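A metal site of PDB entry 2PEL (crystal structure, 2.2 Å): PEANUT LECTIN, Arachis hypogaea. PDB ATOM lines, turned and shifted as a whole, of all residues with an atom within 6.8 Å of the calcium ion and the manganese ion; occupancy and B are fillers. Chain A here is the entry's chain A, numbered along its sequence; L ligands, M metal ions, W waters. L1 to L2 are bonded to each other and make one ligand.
Four residues have an atom within 4 Å of the manganese ion: Glu 121, Asp 123, Asp 132 and His 137.
The nearest printed residue that does not touch the manganese ion is Val 145 (4.3 Å).
The manganese ion is bound by water W1, OD2 of Asp 123, OD1 of Asp 132, OE2 of Glu 121, water W4 and NE2 of His 137.
The manganese ion has six donor atoms within binding distance.
OD2 of Asp 132 is bound to the calcium ion (2.4 Å).
The calcium ion is bound by the side-chain amide oxygen (OD1) of Asn 127, 2.4 Å away.
O of Tyr 125 is bound to the calcium ion (2.4 Å).
Water W2 binds the calcium ion, at 2.4 Å.
The calcium ion is bound by water W3.
The side-chain carboxylate (OD1) of Asp 123 is bound to the calcium ion.
The calcium ion is bound by OD2 of Asp 123, 2.5 Å away.
The calcium ion has seven donor atoms within binding distance.
Water W1 lies within hydrogen-bond range of the backbone carbonyl oxygen (O) of Val 145 (2.7 Å) and the side-chain carboxylate (OE1) of Glu 121 (2.8 Å).
The side-chain carboxylate of Glu 121 is in hydrogen-bond range of the side-chain hydroxyl of Ser 147 (3.4 Å).
OE1 of Glu 121 sits close to OD2 of Asp 141, 2.4 Å away.
The backbone NH (N) of Glu 121 sits at hydrogen-bond distance from the backbone carbonyl oxygen (O) of Gly 139, at 3.1 Å.
An oxygen (O2) of LG2 L2 lies within hydrogen-bond range of the side-chain amide nitrogen (ND2) of Asn 127, 2.9 Å away.
The backbone NH (N) of Gly 104 lies within hydrogen-bond range of an oxygen (O2) of LG2 L2 (3.1 Å).
O3 of LG2 L2 sits at hydrogen-bond distance from OD2 of Asp 83 (2.6 Å).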
ATOM      1  N   ASP A  83       1.218   0.087 -21.161  1.00  0.00           N
ATOM      2  CA  ASP A  83       0.311  -0.942 -20.667  1.00  0.00           C
ATOM      3  C   ASP A  83       0.728  -2.374 -20.993  1.00  0.00           C
ATOM      4  O   ASP A  83       0.164  -3.285 -20.371  1.00  0.00           O
ATOM      5  CB  ASP A  83      -1.054  -0.586 -21.303  1.00  0.00           C
ATOM      6  CG  ASP A  83      -1.858   0.341 -20.404  1.00  0.00           C
ATOM      7  OD1 ASP A  83      -2.604  -0.108 -19.508  1.00  0.00           O
ATOM      8  OD2 ASP A  83      -1.722   1.566 -20.616  1.00  0.00           O
ATOM      9  N   GLY A 103      -4.533   2.430 -23.706  1.00  0.00           N
ATOM     10  CA  GLY A 103      -4.555   1.859 -22.375  1.00  0.00           C
ATOM     11  C   GLY A 103      -4.621   0.334 -22.348  1.00  0.00           C
ATOM     12  O   GLY A 103      -3.931  -0.381 -23.073  1.00  0.00           O
ATOM     13  N   GLY A 104      -5.505  -0.136 -21.454  1.00  0.00           N
ATOM     14  CA  GLY A 104      -5.762  -1.535 -21.161  1.00  0.00           C
ATOM     15  C   GLY A 104      -6.436  -2.362 -22.233  1.00  0.00           C
ATOM     16  O   GLY A 104      -6.699  -3.565 -21.995  1.00  0.00           O
ATOM     17  N   THR A 105      -6.721  -1.729 -23.355  1.00  0.00           N
ATOM     18  CA  THR A 105      -7.374  -2.400 -24.492  1.00  0.00           C
ATOM     19  C   THR A 105      -6.265  -3.007 -25.357  1.00  0.00           C
ATOM     20  O   THR A 105      -6.570  -3.810 -26.251  1.00  0.00           O
ATOM     21  CB  THR A 105      -8.282  -1.469 -25.376  1.00  0.00           C
ATOM     22  OG1 THR A 105      -7.347  -0.508 -25.975  1.00  0.00           O
ATOM     23  CG2 THR A 105      -9.419  -0.686 -24.734  1.00  0.00           C
ATOM     24  N   LEU A 106      -5.042  -2.590 -25.098  1.00  0.00           N
ATOM     25  CA  LEU A 106      -3.814  -3.013 -25.764  1.00  0.00           C
ATOM     26  C   LEU A 106      -3.785  -2.814 -27.281  1.00  0.00           C
ATOM     27  O   LEU A 106      -3.043  -3.486 -28.034  1.00  0.00           O
ATOM     28  CB  LEU A 106      -3.531  -4.481 -25.333  1.00  0.00           C
ATOM     29  CG  LEU A 106      -3.342  -4.750 -23.838  1.00  0.00           C
ATOM     30  CD1 LEU A 106      -3.162  -6.235 -23.525  1.00  0.00           C
ATOM     31  CD2 LEU A 106      -2.101  -3.999 -23.325  1.00  0.00           C
ATOM     32  N   GLU A 121      -0.933 -11.911 -24.043  1.00  0.00           N
ATOM     33  CA  GLU A 121      -0.557 -10.562 -23.535  1.00  0.00           C
ATOM     34  C   GLU A 121       0.485 -10.556 -22.417  1.00  0.00           C
ATOM     35  O   GLU A 121       0.601 -11.477 -21.593  1.00  0.00           O
ATOM     36  CB  GLU A 121      -1.798  -9.868 -22.985  1.00  0.00           C
ATOM     37  CG  GLU A 121      -2.567 -10.603 -21.899  1.00  0.00           C
ATOM     38  CD  GLU A 121      -3.607  -9.732 -21.254  1.00  0.00           C
ATOM     39  OE1 GLU A 121      -4.664  -9.556 -21.837  1.00  0.00           O
ATOM     40  OE2 GLU A 121      -3.266  -9.224 -20.173  1.00  0.00           O
ATOM     41  N   ASP A 123       0.937  -8.212 -19.890  1.00  0.00           N
ATOM     42  CA  ASP A 123       0.252  -7.039 -19.289  1.00  0.00           C
ATOM     43  C   ASP A 123       0.926  -6.443 -18.066  1.00  0.00           C
ATOM     44  O   ASP A 123       0.970  -7.129 -17.042  1.00  0.00           O
ATOM     45  CB  ASP A 123      -1.191  -7.475 -19.090  1.00  0.00           C
ATOM     46  CG  ASP A 123      -2.152  -6.358 -18.804  1.00  0.00           C
ATOM     47  OD1 ASP A 123      -1.762  -5.235 -18.398  1.00  0.00           O
ATOM     48  OD2 ASP A 123      -3.365  -6.587 -18.985  1.00  0.00           O
ATOM     49  N   THR A 124       1.371  -5.187 -18.192  1.00  0.00           N
ATOM     50  CA  THR A 124       2.050  -4.519 -17.074  1.00  0.00           C
ATOM     51  C   THR A 124       1.232  -3.538 -16.259  1.00  0.00           C
ATOM     52  O   THR A 124       1.849  -2.775 -15.472  1.00  0.00           O
ATOM     53  CB  THR A 124       3.356  -3.759 -17.529  1.00  0.00           C
ATOM     54  OG1 THR A 124       2.903  -2.535 -18.186  1.00  0.00           O
ATOM     55  CG2 THR A 124       4.277  -4.598 -18.406  1.00  0.00           C
ATOM     56  N   TYR A 125      -0.067  -3.500 -16.407  1.00  0.00           N
ATOM     57  CA  TYR A 125      -0.874  -2.530 -15.624  1.00  0.00           C
ATOM     58  C   TYR A 125      -2.187  -3.219 -15.283  1.00  0.00           C
ATOM     59  O   TYR A 125      -2.796  -3.801 -16.194  1.00  0.00           O
ATOM     60  CB  TYR A 125      -1.124  -1.194 -16.367  1.00  0.00           C
ATOM     61  CG  TYR A 125      -1.992  -0.316 -15.478  1.00  0.00           C
ATOM     62  CD1 TYR A 125      -3.397  -0.407 -15.564  1.00  0.00           C
ATOM     63  CD2 TYR A 125      -1.412   0.540 -14.536  1.00  0.00           C
ATOM     64  CE1 TYR A 125      -4.197   0.346 -14.715  1.00  0.00           C
ATOM     65  CE2 TYR A 125      -2.213   1.306 -13.686  1.00  0.00           C
ATOM     66  CZ  TYR A 125      -3.598   1.218 -13.794  1.00  0.00           C
ATOM     67  OH  TYR A 125      -4.422   1.957 -12.982  1.00  0.00           O
ATOM     68  N   SER A 126      -2.649  -3.070 -14.062  1.00  0.00           N
ATOM     69  CA  SER A 126      -3.901  -3.728 -13.663  1.00  0.00           C
ATOM     70  C   SER A 126      -5.171  -2.925 -13.827  1.00  0.00           C
ATOM     71  O   SER A 126      -5.439  -2.017 -13.013  1.00  0.00           O
ATOM     72  CB  SER A 126      -3.677  -4.189 -12.221  1.00  0.00           C
ATOM     73  OG  SER A 126      -4.738  -5.035 -11.806  1.00  0.00           O
ATOM     74  N   ASN A 127      -5.953  -3.290 -14.829  1.00  0.00           N
ATOM     75  CA  ASN A 127      -7.227  -2.666 -15.184  1.00  0.00           C
ATOM     76  C   ASN A 127      -8.353  -3.517 -14.586  1.00  0.00           C
ATOM     77  O   ASN A 127      -8.634  -4.598 -15.130  1.00  0.00           O
ATOM     78  CB  ASN A 127      -7.471  -2.544 -16.695  1.00  0.00           C
ATOM     79  CG  ASN A 127      -6.363  -1.775 -17.375  1.00  0.00           C
ATOM     80  OD1 ASN A 127      -5.366  -2.419 -17.756  1.00  0.00           O
ATOM     81  ND2 ASN A 127      -6.459  -0.461 -17.561  1.00  0.00           N
ATOM     82  N   TYR A 130     -11.265  -4.691 -16.759  1.00  0.00           N
ATOM     83  CA  TYR A 130     -11.107  -5.908 -17.584  1.00  0.00           C
ATOM     84  C   TYR A 130     -10.681  -7.061 -16.674  1.00  0.00           C
ATOM     85  O   TYR A 130     -10.047  -7.996 -17.175  1.00  0.00           O
ATOM     86  CB  TYR A 130     -10.085  -5.723 -18.708  1.00  0.00           C
ATOM     87  CG  TYR A 130     -10.338  -4.449 -19.477  1.00  0.00           C
ATOM     88  CD1 TYR A 130     -11.570  -4.238 -20.086  1.00  0.00           C
ATOM     89  CD2 TYR A 130      -9.365  -3.455 -19.572  1.00  0.00           C
ATOM     90  CE1 TYR A 130     -11.818  -3.066 -20.813  1.00  0.00           C
ATOM     91  CE2 TYR A 130      -9.584  -2.295 -20.288  1.00  0.00           C
ATOM     92  CZ  TYR A 130     -10.813  -2.105 -20.912  1.00  0.00           C
ATOM     93  OH  TYR A 130     -11.073  -0.965 -21.601  1.00  0.00           O
ATOM     94  N   ASN A 131     -11.026  -6.953 -15.424  1.00  0.00           N
ATOM     95  CA  ASN A 131     -10.753  -7.937 -14.379  1.00  0.00           C
ATOM     96  C   ASN A 131      -9.301  -8.422 -14.342  1.00  0.00           C
ATOM     97  O   ASN A 131      -9.100  -9.648 -14.237  1.00  0.00           O
ATOM     98  CB  ASN A 131     -11.683  -9.154 -14.495  1.00  0.00           C
ATOM     99  CG  ASN A 131     -13.145  -8.772 -14.398  1.00  0.00           C
ATOM    100  OD1 ASN A 131     -13.532  -7.928 -13.563  1.00  0.00           O
ATOM    101  ND2 ASN A 131     -13.965  -9.416 -15.248  1.00  0.00           N
ATOM    102  N   ASP A 132      -8.352  -7.510 -14.417  1.00  0.00           N
ATOM    103  CA  ASP A 132      -6.954  -7.914 -14.386  1.00  0.00           C
ATOM    104  C   ASP A 132      -6.514  -8.420 -13.017  1.00  0.00           C
ATOM    105  O   ASP A 132      -6.989  -7.888 -12.014  1.00  0.00           O
ATOM    106  CB  ASP A 132      -6.111  -6.671 -14.676  1.00  0.00           C
ATOM    107  CG  ASP A 132      -5.773  -6.515 -16.157  1.00  0.00           C
ATOM    108  OD1 ASP A 132      -6.026  -7.464 -16.910  1.00  0.00           O
ATOM    109  OD2 ASP A 132      -5.289  -5.383 -16.375  1.00  0.00           O
ATOM    110  N   PRO A 133      -5.580  -9.374 -13.021  1.00  0.00           N
ATOM    111  CA  PRO A 133      -5.000  -9.872 -11.769  1.00  0.00           C
ATOM    112  C   PRO A 133      -4.271  -8.627 -11.198  1.00  0.00           C
ATOM    113  O   PRO A 133      -3.944  -7.642 -11.908  1.00  0.00           O
ATOM    114  CB  PRO A 133      -4.066 -10.982 -12.197  1.00  0.00           C
ATOM    115  CG  PRO A 133      -4.544 -11.361 -13.589  1.00  0.00           C
ATOM    116  CD  PRO A 133      -4.967 -10.024 -14.176  1.00  0.00           C
ATOM    117  N   HIS A 137       1.371  -9.767 -15.477  1.00  0.00           N
ATOM    118  CA  HIS A 137       0.953 -11.121 -15.862  1.00  0.00           C
ATOM    119  C   HIS A 137       0.939 -11.427 -17.348  1.00  0.00           C
ATOM    120  O   HIS A 137       0.961 -10.493 -18.157  1.00  0.00           O
ATOM    121  CB  HIS A 137      -0.484 -11.395 -15.311  1.00  0.00           C
ATOM    122  CG  HIS A 137      -1.464 -10.357 -15.774  1.00  0.00           C
ATOM    123  ND1 HIS A 137      -1.541  -9.085 -15.217  1.00  0.00           N
ATOM    124  CD2 HIS A 137      -2.415 -10.434 -16.757  1.00  0.00           C
ATOM    125  CE1 HIS A 137      -2.509  -8.441 -15.837  1.00  0.00           C
ATOM    126  NE2 HIS A 137      -3.047  -9.215 -16.757  1.00  0.00           N
ATOM    127  N   VAL A 138       0.876 -12.726 -17.603  1.00  0.00           N
ATOM    128  CA  VAL A 138       0.782 -13.304 -18.986  1.00  0.00           C
ATOM    129  C   VAL A 138      -0.649 -13.857 -19.021  1.00  0.00           C
ATOM    130  O   VAL A 138      -1.148 -14.430 -18.036  1.00  0.00           O
ATOM    131  CB  VAL A 138       1.883 -14.323 -19.243  1.00  0.00           C
ATOM    132  CG1 VAL A 138       1.917 -14.842 -20.666  1.00  0.00           C
ATOM    133  CG2 VAL A 138       3.276 -13.820 -18.850  1.00  0.00           C
ATOM    134  N   GLY A 139      -1.398 -13.631 -20.088  1.00  0.00           N
ATOM    135  CA  GLY A 139      -2.798 -14.115 -20.151  1.00  0.00           C
ATOM    136  C   GLY A 139      -3.031 -14.581 -21.585  1.00  0.00           C
ATOM    137  O   GLY A 139      -2.285 -14.223 -22.508  1.00  0.00           O
ATOM    138  N   ASP A 141      -5.895 -14.520 -24.352  1.00  0.00           N
ATOM    139  CA  ASP A 141      -7.119 -13.762 -24.630  1.00  0.00           C
ATOM    140  C   ASP A 141      -7.900 -14.314 -25.819  1.00  0.00           C
ATOM    141  O   ASP A 141      -7.237 -14.448 -26.851  1.00  0.00           O
ATOM    142  CB  ASP A 141      -6.714 -12.312 -24.934  1.00  0.00           C
ATOM    143  CG  ASP A 141      -6.076 -11.587 -23.762  1.00  0.00           C
ATOM    144  OD1 ASP A 141      -5.856 -12.208 -22.695  1.00  0.00           O
ATOM    145  OD2 ASP A 141      -5.759 -10.397 -23.836  1.00  0.00           O
ATOM    146  N   VAL A 145     -10.017  -8.668 -23.663  1.00  0.00           N
ATOM    147  CA  VAL A 145      -8.812  -8.439 -22.849  1.00  0.00           C
ATOM    148  C   VAL A 145      -9.105  -8.916 -21.405  1.00  0.00           C
ATOM    149  O   VAL A 145      -8.325  -8.718 -20.458  1.00  0.00           O
ATOM    150  CB  VAL A 145      -8.229  -7.027 -22.871  1.00  0.00           C
ATOM    151  CG1 VAL A 145      -7.358  -6.791 -24.105  1.00  0.00           C
ATOM    152  CG2 VAL A 145      -9.322  -5.998 -22.634  1.00  0.00           C
ATOM    153  N   ASP A 146     -10.256  -9.554 -21.262  1.00  0.00           N
ATOM    154  CA  ASP A 146     -10.697 -10.155 -19.978  1.00  0.00           C
ATOM    155  C   ASP A 146     -10.284 -11.632 -20.275  1.00  0.00           C
ATOM    156  O   ASP A 146     -11.060 -12.433 -20.845  1.00  0.00           O
ATOM    157  CB  ASP A 146     -12.132  -9.932 -19.603  1.00  0.00           C
ATOM    158  CG  ASP A 146     -12.558 -10.542 -18.280  1.00  0.00           C
ATOM    159  OD1 ASP A 146     -11.726 -11.210 -17.622  1.00  0.00           O
ATOM    160  OD2 ASP A 146     -13.724 -10.380 -17.867  1.00  0.00           O
ATOM    161  N   SER A 147      -9.034 -11.859 -19.933  1.00  0.00           N
ATOM    162  CA  SER A 147      -8.367 -13.152 -20.154  1.00  0.00           C
ATOM    163  C   SER A 147      -9.121 -14.357 -19.568  1.00  0.00           C
ATOM    164  O   SER A 147      -9.661 -14.436 -18.463  1.00  0.00           O
ATOM    165  CB  SER A 147      -6.932 -13.183 -19.687  1.00  0.00           C
ATOM    166  OG  SER A 147      -6.101 -12.182 -20.211  1.00  0.00           O
ATOM    167  N   THR A 150      -4.890 -16.468 -16.799  1.00  0.00           N
ATOM    168  CA  THR A 150      -3.675 -15.679 -16.570  1.00  0.00           C
ATOM    169  C   THR A 150      -2.748 -16.375 -15.567  1.00  0.00           C
ATOM    170  O   THR A 150      -3.144 -17.243 -14.805  1.00  0.00           O
ATOM    171  CB  THR A 150      -4.001 -14.224 -16.027  1.00  0.00           C
ATOM    172  OG1 THR A 150      -4.438 -14.519 -14.653  1.00  0.00           O
ATOM    173  CG2 THR A 150      -5.020 -13.437 -16.842  1.00  0.00           C
HETATM  174  C1  LIG L   1      -6.520   9.665 -15.954  1.00  0.00           C
HETATM  175  C2  LIG L   1      -5.047   9.364 -16.175  1.00  0.00           C
HETATM  176  C3  LIG L   1      -4.938   8.243 -17.227  1.00  0.00           C
HETATM  177  C4  LIG L   1      -5.658   7.000 -16.658  1.00  0.00           C
HETATM  178  C5  LIG L   1      -7.109   7.332 -16.345  1.00  0.00           C
HETATM  179  C6  LIG L   1      -7.905   6.265 -15.643  1.00  0.00           C
HETATM  180  O1  LIG L   1      -6.948  10.078 -17.300  1.00  0.00           O
HETATM  181  O2  LIG L   1      -4.403  10.643 -16.552  1.00  0.00           O
HETATM  182  O3  LIG L   1      -3.595   7.790 -17.292  1.00  0.00           O
HETATM  183  O4  LIG L   1      -5.412   5.902 -17.534  1.00  0.00           O
HETATM  184  O5  LIG L   1      -7.169   8.502 -15.524  1.00  0.00           O
HETATM  185  O6  LIG L   1      -7.300   5.854 -14.381  1.00  0.00           O
HETATM  186  C1  LG2 L   2      -4.968   4.672 -17.019  1.00  0.00           C
HETATM  187  C2  LG2 L   2      -5.229   3.646 -18.125  1.00  0.00           C
HETATM  188  C3  LG2 L   2      -4.471   2.373 -17.891  1.00  0.00           C
HETATM  189  C4  LG2 L   2      -2.998   2.640 -17.665  1.00  0.00           C
HETATM  190  C5  LG2 L   2      -2.895   3.580 -16.471  1.00  0.00           C
HETATM  191  C6  LG2 L   2      -1.492   3.982 -16.138  1.00  0.00           C
HETATM  192  O1  LG2 L   2      -6.595   3.437 -18.315  1.00  0.00           O
HETATM  193  O2  LG2 L   2      -4.736   1.390 -18.899  1.00  0.00           O
HETATM  194  O3  LG2 L   2      -2.268   3.263 -18.734  1.00  0.00           O
HETATM  195  O4  LG2 L   2      -3.584   4.822 -16.782  1.00  0.00           O
HETATM  196  O5  LG2 L   2      -1.573   4.942 -15.100  1.00  0.00           O
HETATM  197 CA    CA M   1      -4.047  -4.376 -18.155  1.00  0.00          CA
HETATM  198 MN    MN M   2      -4.565  -8.463 -18.397  1.00  0.00          MN
HETATM  199  O   HOH W   1      -5.836  -7.638 -20.131  1.00  0.00           O
HETATM  200  O   HOH W   2      -2.599  -2.913 -19.418  1.00  0.00           O
HETATM  201  O   HOH W   3      -5.593  -5.037 -19.904  1.00  0.00           O
HETATM  202  O   HOH W   4      -5.924 -10.359 -18.282  1.00  0.00           O
